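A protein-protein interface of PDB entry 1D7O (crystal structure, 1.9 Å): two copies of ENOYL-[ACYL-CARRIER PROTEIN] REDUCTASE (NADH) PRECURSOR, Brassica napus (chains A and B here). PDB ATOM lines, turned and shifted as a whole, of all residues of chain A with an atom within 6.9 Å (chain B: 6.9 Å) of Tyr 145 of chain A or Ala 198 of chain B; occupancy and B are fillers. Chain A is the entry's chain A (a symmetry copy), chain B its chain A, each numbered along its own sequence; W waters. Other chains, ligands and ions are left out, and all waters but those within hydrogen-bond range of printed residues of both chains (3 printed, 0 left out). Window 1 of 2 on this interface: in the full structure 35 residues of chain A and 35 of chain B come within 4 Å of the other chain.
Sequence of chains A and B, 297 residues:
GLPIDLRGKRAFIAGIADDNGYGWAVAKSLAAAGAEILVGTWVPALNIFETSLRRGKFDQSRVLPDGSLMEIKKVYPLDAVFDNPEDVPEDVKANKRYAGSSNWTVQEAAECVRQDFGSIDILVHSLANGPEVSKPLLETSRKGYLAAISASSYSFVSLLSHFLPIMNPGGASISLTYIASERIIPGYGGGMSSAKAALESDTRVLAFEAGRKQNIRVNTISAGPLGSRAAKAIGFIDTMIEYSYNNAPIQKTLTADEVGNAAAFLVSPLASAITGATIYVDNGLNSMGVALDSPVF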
ATOM      1  N   PRO A 131      17.129 -18.163 -17.233  1.00  0.00           N
ATOM      2  CA  PRO A 131      16.306 -18.124 -16.028  1.00  0.00           C
ATOM      3  C   PRO A 131      16.898 -17.397 -14.816  1.00  0.00           C
ATOM      4  O   PRO A 131      16.145 -16.785 -14.056  1.00  0.00           O
ATOM      5  CB  PRO A 131      16.123 -19.607 -15.673  1.00  0.00           C
ATOM      6  CG  PRO A 131      17.278 -20.307 -16.341  1.00  0.00           C
ATOM      7  CD  PRO A 131      17.459 -19.537 -17.636  1.00  0.00           C
ATOM      8  N   GLU A 132      18.221 -17.469 -14.607  1.00  0.00           N
ATOM      9  CA  GLU A 132      18.862 -16.815 -13.448  1.00  0.00           C
ATOM     10  C   GLU A 132      19.629 -15.547 -13.757  1.00  0.00           C
ATOM     11  O   GLU A 132      20.516 -15.164 -13.018  1.00  0.00           O
ATOM     12  CB  GLU A 132      19.698 -17.821 -12.664  1.00  0.00           C
ATOM     13  CG  GLU A 132      18.816 -18.988 -12.115  1.00  0.00           C
ATOM     14  CD  GLU A 132      19.564 -20.000 -11.275  1.00  0.00           C
ATOM     15  OE1 GLU A 132      20.592 -19.665 -10.690  1.00  0.00           O
ATOM     16  OE2 GLU A 132      19.217 -21.181 -11.315  1.00  0.00           O
ATOM     17  N   LEU A 137      27.012 -14.440 -10.675  1.00  0.00           N
ATOM     18  CA  LEU A 137      27.502 -15.764 -10.950  1.00  0.00           C
ATOM     19  C   LEU A 137      27.727 -16.553  -9.674  1.00  0.00           C
ATOM     20  O   LEU A 137      27.528 -17.760  -9.657  1.00  0.00           O
ATOM     21  CB  LEU A 137      28.835 -15.730 -11.702  1.00  0.00           C
ATOM     22  CG  LEU A 137      28.857 -15.753 -13.217  1.00  0.00           C
ATOM     23  CD1 LEU A 137      30.338 -15.959 -13.585  1.00  0.00           C
ATOM     24  CD2 LEU A 137      27.981 -16.871 -13.771  1.00  0.00           C
ATOM     25  N   THR A 140      24.509 -18.329  -8.991  1.00  0.00           N
ATOM     26  CA  THR A 140      23.817 -19.037 -10.052  1.00  0.00           C
ATOM     27  C   THR A 140      23.992 -20.511  -9.910  1.00  0.00           C
ATOM     28  O   THR A 140      25.081 -20.957  -9.646  1.00  0.00           O
ATOM     29  CB  THR A 140      24.374 -18.596 -11.430  1.00  0.00           C
ATOM     30  OG1 THR A 140      24.079 -17.205 -11.627  1.00  0.00           O
ATOM     31  CG2 THR A 140      23.744 -19.407 -12.554  1.00  0.00           C
ATOM     32  N   SER A 141      22.920 -21.274 -10.087  1.00  0.00           N
ATOM     33  CA  SER A 141      23.002 -22.734  -9.957  1.00  0.00           C
ATOM     34  C   SER A 141      23.512 -23.368 -11.217  1.00  0.00           C
ATOM     35  O   SER A 141      23.469 -22.770 -12.312  1.00  0.00           O
ATOM     36  CB  SER A 141      21.627 -23.338  -9.659  1.00  0.00           C
ATOM     37  OG  SER A 141      20.777 -23.185 -10.785  1.00  0.00           O
ATOM     38  N   ARG A 142      23.945 -24.610 -11.068  1.00  0.00           N
ATOM     39  CA  ARG A 142      24.452 -25.315 -12.218  1.00  0.00           C
ATOM     40  C   ARG A 142      23.351 -25.429 -13.280  1.00  0.00           C
ATOM     41  O   ARG A 142      23.570 -25.206 -14.491  1.00  0.00           O
ATOM     42  CB  ARG A 142      24.993 -26.670 -11.814  1.00  0.00           C
ATOM     43  CG  ARG A 142      25.584 -27.405 -12.985  1.00  0.00           C
ATOM     44  CD  ARG A 142      26.219 -28.752 -12.541  1.00  0.00           C
ATOM     45  NE  ARG A 142      27.214 -28.572 -11.495  1.00  0.00           N
ATOM     46  CZ  ARG A 142      28.533 -28.640 -11.679  1.00  0.00           C
ATOM     47  NH1 ARG A 142      29.020 -28.896 -12.895  1.00  0.00           N
ATOM     48  NH2 ARG A 142      29.357 -28.446 -10.634  1.00  0.00           N
ATOM     49  N   LYS A 143      22.137 -25.734 -12.844  1.00  0.00           N
ATOM     50  CA  LYS A 143      21.048 -25.844 -13.820  1.00  0.00           C
ATOM     51  C   LYS A 143      20.771 -24.504 -14.496  1.00  0.00           C
ATOM     52  O   LYS A 143      20.531 -24.431 -15.694  1.00  0.00           O
ATOM     53  CB  LYS A 143      19.730 -26.358 -13.118  1.00  0.00           C
ATOM     54  N   GLY A 144      20.784 -23.433 -13.713  1.00  0.00           N
ATOM     55  CA  GLY A 144      20.491 -22.136 -14.298  1.00  0.00           C
ATOM     56  C   GLY A 144      21.546 -21.790 -15.338  1.00  0.00           C
ATOM     57  O   GLY A 144      21.223 -21.310 -16.427  1.00  0.00           O
ATOM     58  N   TYR A 145      22.805 -22.006 -14.981  1.00  0.00           N
ATOM     59  CA  TYR A 145      23.883 -21.679 -15.895  1.00  0.00           C
ATOM     60  C   TYR A 145      23.818 -22.535 -17.173  1.00  0.00           C
ATOM     61  O   TYR A 145      23.900 -22.034 -18.310  1.00  0.00           O
ATOM     62  CB  TYR A 145      25.159 -21.824 -15.095  1.00  0.00           C
ATOM     63  CG  TYR A 145      26.519 -21.562 -15.726  1.00  0.00           C
ATOM     64  CD1 TYR A 145      27.118 -22.509 -16.568  1.00  0.00           C
ATOM     65  CD2 TYR A 145      27.250 -20.404 -15.392  1.00  0.00           C
ATOM     66  CE1 TYR A 145      28.424 -22.317 -17.065  1.00  0.00           C
ATOM     67  CE2 TYR A 145      28.550 -20.201 -15.873  1.00  0.00           C
ATOM     68  CZ  TYR A 145      29.130 -21.153 -16.704  1.00  0.00           C
ATOM     69  OH  TYR A 145      30.407 -20.958 -17.175  1.00  0.00           O
ATOM     70  N   LEU A 146      23.620 -23.833 -17.009  1.00  0.00           N
ATOM     71  CA  LEU A 146      23.551 -24.663 -18.192  1.00  0.00           C
ATOM     72  C   LEU A 146      22.353 -24.325 -19.018  1.00  0.00           C
ATOM     73  O   LEU A 146      22.369 -24.520 -20.225  1.00  0.00           O
ATOM     74  CB  LEU A 146      23.575 -26.159 -17.845  1.00  0.00           C
ATOM     75  CG  LEU A 146      24.888 -26.580 -17.216  1.00  0.00           C
ATOM     76  CD1 LEU A 146      24.719 -28.009 -16.792  1.00  0.00           C
ATOM     77  CD2 LEU A 146      26.049 -26.480 -18.236  1.00  0.00           C
ATOM     78  N   ALA A 147      21.288 -23.837 -18.383  1.00  0.00           N
ATOM     79  CA  ALA A 147      20.084 -23.488 -19.157  1.00  0.00           C
ATOM     80  C   ALA A 147      20.387 -22.277 -20.052  1.00  0.00           C
ATOM     81  O   ALA A 147      19.945 -22.199 -21.200  1.00  0.00           O
ATOM     82  CB  ALA A 147      18.887 -23.143 -18.200  1.00  0.00           C
ATOM     83  N   ALA A 148      21.134 -21.318 -19.517  1.00  0.00           N
ATOM     84  CA  ALA A 148      21.466 -20.136 -20.296  1.00  0.00           C
ATOM     85  C   ALA A 148      22.333 -20.533 -21.505  1.00  0.00           C
ATOM     86  O   ALA A 148      22.154 -20.041 -22.621  1.00  0.00           O
ATOM     87  CB  ALA A 148      22.156 -19.112 -19.406  1.00  0.00           C
ATOM     88  N   ILE A 149      23.267 -21.434 -21.252  1.00  0.00           N
ATOM     89  CA  ILE A 149      24.148 -21.881 -22.301  1.00  0.00           C
ATOM     90  C   ILE A 149      23.371 -22.666 -23.329  1.00  0.00           C
ATOM     91  O   ILE A 149      23.561 -22.541 -24.545  1.00  0.00           O
ATOM     92  CB  ILE A 149      25.197 -22.854 -21.760  1.00  0.00           C
ATOM     93  CG1 ILE A 149      26.052 -22.228 -20.650  1.00  0.00           C
ATOM     94  CG2 ILE A 149      26.080 -23.373 -22.897  1.00  0.00           C
ATOM     95  CD1 ILE A 149      26.685 -20.970 -21.015  1.00  0.00           C
ATOM     96  N   SER A 150      22.495 -23.522 -22.860  1.00  0.00           N
ATOM     97  CA  SER A 150      21.754 -24.330 -23.808  1.00  0.00           C
ATOM     98  C   SER A 150      20.858 -23.490 -24.732  1.00  0.00           C
ATOM     99  O   SER A 150      20.809 -23.701 -25.946  1.00  0.00           O
ATOM    100  CB  SER A 150      20.935 -25.384 -23.068  1.00  0.00           C
ATOM    101  OG  SER A 150      20.195 -26.147 -23.996  1.00  0.00           O
ATOM    102  N   GLY A 190      23.502 -14.870 -14.189  1.00  0.00           N
ATOM    103  CA  GLY A 190      23.003 -16.201 -14.493  1.00  0.00           C
ATOM    104  C   GLY A 190      23.719 -16.991 -15.585  1.00  0.00           C
ATOM    105  O   GLY A 190      23.155 -17.927 -16.119  1.00  0.00           O
ATOM    106  N   GLY A 191      24.963 -16.639 -15.905  1.00  0.00           N
ATOM    107  CA  GLY A 191      25.710 -17.377 -16.921  1.00  0.00           C
ATOM    108  C   GLY A 191      25.427 -16.832 -18.292  1.00  0.00           C
ATOM    109  O   GLY A 191      25.843 -17.438 -19.282  1.00  0.00           O
ATOM    110  N   MET A 192      24.698 -15.714 -18.376  1.00  0.00           N
ATOM    111  CA  MET A 192      24.435 -15.144 -19.704  1.00  0.00           C
ATOM    112  C   MET A 192      25.765 -14.588 -20.262  1.00  0.00           C
ATOM    113  O   MET A 192      26.021 -14.686 -21.468  1.00  0.00           O
ATOM    114  CB  MET A 192      23.366 -14.044 -19.674  1.00  0.00           C
ATOM    115  CG  MET A 192      21.931 -14.560 -19.670  1.00  0.00           C
ATOM    116  SD  MET A 192      21.573 -15.559 -21.157  1.00  0.00           S
ATOM    117  CE  MET A 192      22.144 -14.492 -22.349  1.00  0.00           C
ATOM    118  N   SER A 193      26.624 -14.052 -19.384  1.00  0.00           N
ATOM    119  CA  SER A 193      27.915 -13.545 -19.871  1.00  0.00           C
ATOM    120  C   SER A 193      28.696 -14.752 -20.432  1.00  0.00           C
ATOM    121  O   SER A 193      29.337 -14.695 -21.496  1.00  0.00           O
ATOM    122  CB  SER A 193      28.718 -12.902 -18.741  1.00  0.00           C
ATOM    123  OG  SER A 193      28.870 -13.761 -17.624  1.00  0.00           O
ATOM    124  N   SER A 194      28.615 -15.854 -19.692  1.00  0.00           N
ATOM    125  CA  SER A 194      29.289 -17.079 -20.082  1.00  0.00           C
ATOM    126  C   SER A 194      28.776 -17.550 -21.419  1.00  0.00           C
ATOM    127  O   SER A 194      29.548 -17.977 -22.280  1.00  0.00           O
ATOM    128  CB  SER A 194      29.029 -18.131 -19.011  1.00  0.00           C
ATOM    129  OG  SER A 194      29.050 -17.475 -17.748  1.00  0.00           O
ATOM    130  N   ALA A 195      27.472 -17.466 -21.607  1.00  0.00           N
ATOM    131  CA  ALA A 195      26.880 -17.915 -22.859  1.00  0.00           C
ATOM    132  C   ALA A 195      27.291 -17.064 -24.025  1.00  0.00           C
ATOM    133  O   ALA A 195      27.534 -17.583 -25.114  1.00  0.00           O
ATOM    134  CB  ALA A 195      25.360 -17.976 -22.754  1.00  0.00           C
ATOM    135  N   ALA A 197      30.098 -15.492 -24.303  1.00  0.00           N
ATOM    136  CA  ALA A 197      31.491 -15.787 -24.618  1.00  0.00           C
ATOM    137  C   ALA A 197      31.536 -17.076 -25.450  1.00  0.00           C
ATOM    138  O   ALA A 197      32.286 -17.175 -26.420  1.00  0.00           O
ATOM    139  CB  ALA A 197      32.319 -15.968 -23.329  1.00  0.00           C
ATOM    140  N   ALA A 198      30.732 -18.077 -25.093  1.00  0.00           N
ATOM    141  CA  ALA A 198      30.746 -19.338 -25.846  1.00  0.00           C
ATOM    142  C   ALA A 198      30.235 -19.066 -27.267  1.00  0.00           C
ATOM    143  O   ALA A 198      30.789 -19.575 -28.242  1.00  0.00           O
ATOM    144  CB  ALA A 198      29.853 -20.367 -25.151  1.00  0.00           C
ATOM    145  N   SER A 201      32.999 -17.525 -29.391  1.00  0.00           N
ATOM    146  CA  SER A 201      34.068 -18.473 -29.684  1.00  0.00           C
ATOM    147  C   SER A 201      33.541 -19.472 -30.746  1.00  0.00           C
ATOM    148  O   SER A 201      34.254 -19.863 -31.675  1.00  0.00           O
ATOM    149  CB  SER A 201      34.432 -19.213 -28.380  1.00  0.00           C
ATOM    150  OG  SER A 201      35.415 -20.215 -28.599  1.00  0.00           O
ATOM    151  N   LEU B 146      27.038 -29.633 -23.367  1.00  0.00           N
ATOM    152  CA  LEU B 146      26.755 -29.192 -22.018  1.00  0.00           C
ATOM    153  C   LEU B 146      27.597 -29.923 -21.025  1.00  0.00           C
ATOM    154  O   LEU B 146      27.883 -29.394 -19.959  1.00  0.00           O
ATOM    155  CB  LEU B 146      25.264 -29.318 -21.674  1.00  0.00           C
ATOM    156  CG  LEU B 146      24.403 -28.399 -22.516  1.00  0.00           C
ATOM    157  CD1 LEU B 146      22.977 -28.732 -22.189  1.00  0.00           C
ATOM    158  CD2 LEU B 146      24.675 -26.913 -22.171  1.00  0.00           C
ATOM    159  N   ILE B 149      30.908 -28.145 -20.780  1.00  0.00           N
ATOM    160  CA  ILE B 149      30.747 -26.901 -20.070  1.00  0.00           C
ATOM    161  C   ILE B 149      30.574 -27.165 -18.595  1.00  0.00           C
ATOM    162  O   ILE B 149      31.122 -26.476 -17.726  1.00  0.00           O
ATOM    163  CB  ILE B 149      29.469 -26.182 -20.503  1.00  0.00           C
ATOM    164  CG1 ILE B 149      29.452 -25.881 -22.008  1.00  0.00           C
ATOM    165  CG2 ILE B 149      29.276 -24.898 -19.691  1.00  0.00           C
ATOM    166  CD1 ILE B 149      30.615 -25.153 -22.489  1.00  0.00           C
ATOM    167  N   SER B 150      29.779 -28.158 -18.277  1.00  0.00           N
ATOM    168  CA  SER B 150      29.547 -28.425 -16.870  1.00  0.00           C
ATOM    169  C   SER B 150      30.827 -28.841 -16.127  1.00  0.00           C
ATOM    170  O   SER B 150      31.112 -28.369 -15.025  1.00  0.00           O
ATOM    171  CB  SER B 150      28.457 -29.481 -16.712  1.00  0.00           C
ATOM    172  OG  SER B 150      28.260 -29.755 -15.342  1.00  0.00           O
ATOM    173  N   SER B 153      33.853 -25.607 -17.063  1.00  0.00           N
ATOM    174  CA  SER B 153      33.647 -24.176 -16.791  1.00  0.00           C
ATOM    175  C   SER B 153      32.829 -24.011 -15.525  1.00  0.00           C
ATOM    176  O   SER B 153      33.294 -23.417 -14.558  1.00  0.00           O
ATOM    177  CB  SER B 153      32.856 -23.440 -17.912  1.00  0.00           C
ATOM    178  OG  SER B 153      33.149 -23.948 -19.188  1.00  0.00           O
ATOM    179  N   TYR B 154      31.607 -24.524 -15.503  1.00  0.00           N
ATOM    180  CA  TYR B 154      30.823 -24.350 -14.284  1.00  0.00           C
ATOM    181  C   TYR B 154      31.513 -24.962 -13.044  1.00  0.00           C
ATOM    182  O   TYR B 154      31.391 -24.447 -11.945  1.00  0.00           O
ATOM    183  CB  TYR B 154      29.411 -24.900 -14.405  1.00  0.00           C
ATOM    184  CG  TYR B 154      28.621 -24.478 -13.194  1.00  0.00           C
ATOM    185  CD1 TYR B 154      28.090 -23.185 -13.112  1.00  0.00           C
ATOM    186  CD2 TYR B 154      28.471 -25.330 -12.108  1.00  0.00           C
ATOM    187  CE1 TYR B 154      27.410 -22.777 -11.989  1.00  0.00           C
ATOM    188  CE2 TYR B 154      27.778 -24.917 -10.995  1.00  0.00           C
ATOM    189  CZ  TYR B 154      27.257 -23.646 -10.933  1.00  0.00           C
ATOM    190  OH  TYR B 154      26.580 -23.217  -9.806  1.00  0.00           O
ATOM    191  N   SER B 155      32.250 -26.049 -13.199  1.00  0.00           N
ATOM    192  CA  SER B 155      32.919 -26.618 -12.022  1.00  0.00           C
ATOM    193  C   SER B 155      33.749 -25.537 -11.302  1.00  0.00           C
ATOM    194  O   SER B 155      33.906 -25.597 -10.083  1.00  0.00           O
ATOM    195  CB  SER B 155      33.855 -27.757 -12.424  1.00  0.00           C
ATOM    196  OG  SER B 155      34.725 -27.360 -13.472  1.00  0.00           O
ATOM    197  N   VAL B 157      33.082 -22.230 -11.225  1.00  0.00           N
ATOM    198  CA  VAL B 157      32.148 -21.366 -10.503  1.00  0.00           C
ATOM    199  C   VAL B 157      31.678 -22.040  -9.187  1.00  0.00           C
ATOM    200  O   VAL B 157      31.554 -21.426  -8.126  1.00  0.00           O
ATOM    201  CB  VAL B 157      30.929 -21.037 -11.371  1.00  0.00           C
ATOM    202  CG1 VAL B 157      29.904 -20.256 -10.540  1.00  0.00           C
ATOM    203  CG2 VAL B 157      31.356 -20.288 -12.699  1.00  0.00           C
ATOM    204  N   SER B 181      39.888 -21.016 -27.030  1.00  0.00           N
ATOM    205  CA  SER B 181      38.757 -20.189 -26.693  1.00  0.00           C
ATOM    206  C   SER B 181      38.708 -18.922 -27.611  1.00  0.00           C
ATOM    207  O   SER B 181      37.643 -18.439 -27.978  1.00  0.00           O
ATOM    208  CB  SER B 181      38.960 -19.686 -25.274  1.00  0.00           C
ATOM    209  OG  SER B 181      40.178 -18.969 -25.215  1.00  0.00           O
ATOM    210  N   MET B 192      34.714 -28.074 -26.122  1.00  0.00           N
ATOM    211  CA  MET B 192      35.790 -27.746 -25.177  1.00  0.00           C
ATOM    212  C   MET B 192      36.266 -26.305 -25.470  1.00  0.00           C
ATOM    213  O   MET B 192      36.596 -25.560 -24.540  1.00  0.00           O
ATOM    214  CB  MET B 192      36.967 -28.726 -25.259  1.00  0.00           C
ATOM    215  CG  MET B 192      36.760 -30.026 -24.488  1.00  0.00           C
ATOM    216  SD  MET B 192      36.494 -29.717 -22.707  1.00  0.00           S
ATOM    217  CE  MET B 192      37.815 -28.692 -22.407  1.00  0.00           C
ATOM    218  N   SER B 193      36.257 -25.902 -26.748  1.00  0.00           N
ATOM    219  CA  SER B 193      36.669 -24.527 -27.063  1.00  0.00           C
ATOM    220  C   SER B 193      35.651 -23.581 -26.390  1.00  0.00           C
ATOM    221  O   SER B 193      35.996 -22.547 -25.790  1.00  0.00           O
ATOM    222  CB  SER B 193      36.669 -24.281 -28.571  1.00  0.00           C
ATOM    223  OG  SER B 193      35.433 -24.620 -29.178  1.00  0.00           O
ATOM    224  N   SER B 194      34.383 -23.969 -26.495  1.00  0.00           N
ATOM    225  CA  SER B 194      33.302 -23.194 -25.914  1.00  0.00           C
ATOM    226  C   SER B 194      33.485 -23.088 -24.421  1.00  0.00           C
ATOM    227  O   SER B 194      33.290 -22.024 -23.832  1.00  0.00           O
ATOM    228  CB  SER B 194      31.985 -23.886 -26.242  1.00  0.00           C
ATOM    229  OG  SER B 194      32.088 -24.405 -27.563  1.00  0.00           O
ATOM    230  N   ALA B 195      33.871 -24.188 -23.801  1.00  0.00           N
ATOM    231  CA  ALA B 195      34.055 -24.190 -22.356  1.00  0.00           C
ATOM    232  C   ALA B 195      35.199 -23.322 -21.923  1.00  0.00           C
ATOM    233  O   ALA B 195      35.105 -22.638 -20.904  1.00  0.00           O
ATOM    234  CB  ALA B 195      34.235 -25.610 -21.830  1.00  0.00           C
ATOM    235  N   LYS B 196      36.295 -23.346 -22.672  1.00  0.00           N
ATOM    236  CA  LYS B 196      37.404 -22.487 -22.277  1.00  0.00           C
ATOM    237  C   LYS B 196      37.021 -20.994 -22.433  1.00  0.00           C
ATOM    238  O   LYS B 196      37.433 -20.144 -21.627  1.00  0.00           O
ATOM    239  CB  LYS B 196      38.664 -22.816 -23.067  1.00  0.00           C
ATOM    240  CG  LYS B 196      39.235 -24.183 -22.719  1.00  0.00           C
ATOM    241  CD  LYS B 196      39.468 -24.343 -21.228  1.00  0.00           C
ATOM    242  CE  LYS B 196      40.338 -25.623 -20.995  1.00  0.00           C
ATOM    243  NZ  LYS B 196      40.693 -25.827 -19.549  1.00  0.00           N
ATOM    244  N   ALA B 197      36.219 -20.663 -23.447  1.00  0.00           N
ATOM    245  CA  ALA B 197      35.820 -19.269 -23.601  1.00  0.00           C
ATOM    246  C   ALA B 197      34.966 -18.874 -22.387  1.00  0.00           C
ATOM    247  O   ALA B 197      35.115 -17.783 -21.840  1.00  0.00           O
ATOM    248  CB  ALA B 197      35.009 -19.069 -24.897  1.00  0.00           C
ATOM    249  N   ALA B 198      34.069 -19.754 -21.943  1.00  0.00           N
ATOM    250  CA  ALA B 198      33.216 -19.421 -20.794  1.00  0.00           C
ATOM    251  C   ALA B 198      34.103 -19.277 -19.550  1.00  0.00           C
ATOM    252  O   ALA B 198      33.917 -18.361 -18.750  1.00  0.00           O
ATOM    253  CB  ALA B 198      32.179 -20.524 -20.581  1.00  0.00           C
ATOM    254  N   LEU B 199      35.056 -20.195 -19.370  1.00  0.00           N
ATOM    255  CA  LEU B 199      35.907 -20.115 -18.184  1.00  0.00           C
ATOM    256  C   LEU B 199      36.664 -18.787 -18.143  1.00  0.00           C
ATOM    257  O   LEU B 199      36.806 -18.179 -17.085  1.00  0.00           O
ATOM    258  CB  LEU B 199      36.906 -21.264 -18.189  1.00  0.00           C
ATOM    259  CG  LEU B 199      37.996 -21.322 -17.116  1.00  0.00           C
ATOM    260  CD1 LEU B 199      37.330 -21.777 -15.867  1.00  0.00           C
ATOM    261  CD2 LEU B 199      39.090 -22.309 -17.506  1.00  0.00           C
ATOM    262  N   GLU B 200      37.159 -18.332 -19.297  1.00  0.00           N
ATOM    263  CA  GLU B 200      37.915 -17.061 -19.284  1.00  0.00           C
ATOM    264  C   GLU B 200      37.027 -15.861 -18.989  1.00  0.00           C
ATOM    265  O   GLU B 200      37.414 -14.939 -18.279  1.00  0.00           O
ATOM    266  CB  GLU B 200      38.707 -16.870 -20.569  1.00  0.00           C
ATOM    267  CG  GLU B 200      39.763 -17.966 -20.801  1.00  0.00           C
ATOM    268  CD  GLU B 200      40.423 -17.844 -22.177  1.00  0.00           C
ATOM    269  OE1 GLU B 200      40.345 -16.753 -22.764  1.00  0.00           O
ATOM    270  OE2 GLU B 200      40.988 -18.822 -22.708  1.00  0.00           O
ATOM    271  N   SER B 201      35.813 -15.872 -19.534  1.00  0.00           N
ATOM    272  CA  SER B 201      34.875 -14.780 -19.302  1.00  0.00           C
ATOM    273  C   SER B 201      34.475 -14.805 -17.804  1.00  0.00           C
ATOM    274  O   SER B 201      34.350 -13.763 -17.152  1.00  0.00           O
ATOM    275  CB  SER B 201      33.636 -15.006 -20.195  1.00  0.00           C
ATOM    276  OG  SER B 201      32.636 -14.024 -19.968  1.00  0.00           O
ATOM    277  N   ASP B 202      34.267 -16.006 -17.256  1.00  0.00           N
ATOM    278  CA  ASP B 202      33.882 -16.134 -15.821  1.00  0.00           C
ATOM    279  C   ASP B 202      35.014 -15.683 -14.916  1.00  0.00           C
ATOM    280  O   ASP B 202      34.805 -15.211 -13.809  1.00  0.00           O
ATOM    281  CB  ASP B 202      33.465 -17.569 -15.418  1.00  0.00           C
ATOM    282  CG  ASP B 202      32.163 -18.015 -16.080  1.00  0.00           C
ATOM    283  OD1 ASP B 202      31.485 -17.174 -16.734  1.00  0.00           O
ATOM    284  OD2 ASP B 202      31.900 -19.255 -16.057  1.00  0.00           O
ATOM    285  N   THR B 203      36.232 -15.845 -15.388  1.00  0.00           N
ATOM    286  CA  THR B 203      37.376 -15.429 -14.597  1.00  0.00           C
ATOM    287  C   THR B 203      37.283 -13.935 -14.358  1.00  0.00           C
ATOM    288  O   THR B 203      37.530 -13.456 -13.278  1.00  0.00           O
ATOM    289  CB  THR B 203      38.686 -15.731 -15.344  1.00  0.00           C
ATOM    290  OG1 THR B 203      38.794 -17.151 -15.519  1.00  0.00           O
ATOM    291  CG2 THR B 203      39.923 -15.139 -14.599  1.00  0.00           C
ATOM    292  N   ARG B 204      36.922 -13.196 -15.392  1.00  0.00           N
ATOM    293  CA  ARG B 204      36.798 -11.759 -15.279  1.00  0.00           C
ATOM    294  C   ARG B 204      35.646 -11.400 -14.363  1.00  0.00           C
ATOM    295  O   ARG B 204      35.797 -10.651 -13.403  1.00  0.00           O
ATOM    296  CB  ARG B 204      36.544 -11.173 -16.667  1.00  0.00           C
ATOM    297  CG  ARG B 204      37.815 -11.222 -17.539  1.00  0.00           C
ATOM    298  CD  ARG B 204      37.598 -10.531 -18.871  1.00  0.00           C
ATOM    299  NE  ARG B 204      36.765 -11.301 -19.789  1.00  0.00           N
ATOM    300  CZ  ARG B 204      37.235 -12.255 -20.588  1.00  0.00           C
ATOM    301  NH1 ARG B 204      38.536 -12.524 -20.558  1.00  0.00           N
ATOM    302  NH2 ARG B 204      36.419 -12.938 -21.408  1.00  0.00           N
HETATM  303  O   HOH W   1      31.192 -14.688 -17.470  1.00  0.00           O
HETATM  304  O   HOH W   2      34.114 -22.584 -29.804  1.00  0.00           O
HETATM  305  O   HOH W   3      37.494 -19.522 -31.069  1.00  0.00           O
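OH of Tyr 154 of chain B lies within hydrogen-bond range of O of Thr 140 of chain A (2.7 Å). OD1 of Asp 202 of chain B is in hydrogen-bond range of OG of Ser 194 of chain A, at 2.7 Å. The guanidinium group of Arg 142 of chain A sits at hydrogen-bond distance from the side-chain hydroxyl of Ser 150 of chain B. The backbone carbonyl oxygen of Ser 181 of chain B sits at hydrogen-bond distance from the side-chain hydroxyl of Ser 201 of chain A, 2.9 Å away. OH of Tyr 154 of chain B sits at hydrogen-bond distance from N of Arg 142 of chain A, 3.2 Å away. OD2 of Asp 202 of chain B lies within hydrogen-bond range of OH of Tyr 145 of chain A (2.5 Å).
The backbone carbonyl oxygen (O) of Ile 149 of chain B sits at hydrogen-bond distance from the backbone NH (N) of Tyr 154 of chain B (3.0 Å).
Among the printed residues, merely in contact across the chains: Ser 141 of chain A with Tyr 154 of chain B, Tyr 145 of chain A with Tyr 154 of chain B, Ala 197 of chain A with Ser 201 of chain B, Ser 201 of chain A with Ala 197 of chain B, Leu 137 of chain A with Val 157 of chain B, Tyr 145 of chain A with Ser 153 of chain B, Leu 137 of chain A with Asp 202 of chain B, Ala 197 of chain A with Ala 197 of chain B, Ser 201 of chain A with Ser 193 of chain B, Ser 193 of chain A with Ser 201 of chain B, Tyr 145 of chain A with Ile 149 of chain B, Leu 146 of chain A with Leu 146 of chain B, Tyr 145 of chain A with Ala 198 of chain B, Ile 149 of chain A with Leu 146 of chain B and Leu 146 of chain A with Ile 149 of chain B.
Ala 198 of chain B touches one residue of chain A. No residue of chain B comes within 4 Å of Gly 144 of chain A. Of the printed residues of chain B, Ser 194 of chain A touches Asp 202 (2.7 Å). Of the printed residues of chain B, Arg 142 of chain A touches Ser 150 and Tyr 154.
Printed residues of chain B that touch a printed residue of chain A: Leu 146, Ile 149, Ser 150, Ser 153, Tyr 154, Val 157, Ser 181, Ser 193, Ala 197, Ala 198, Ser 201 and Asp 202. Hydrophobic or aromatic side chains of chain B within 4 Å of the printed part of chain A: Leu 146, Ile 149, Tyr 154, Val 157, Ala 197 and Ala 198. Among the printed residues, no Asp or Glu carboxylate lies within 4 Å of a Lys or Arg side-chain nitrogen of the other chain.
Leu 146 of chain A touches its own counterpart, Leu 146 of chain B. Of the 21 pairs that touch across the chains among the printed residues, 8 have their exchanged pair printed and touching as well.
Water W1 lies within hydrogen-bond range of OG of Ser 193 of chain A (2.5 Å), OD1 of Asp 202 of chain B (2.6 Å) and OG of Ser 201 of chain B (3.0 Å). Water W3 bridges O of Ser 181 of chain B (3.3 Å) and OG of Ser 201 of chain A (3.3 Å).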
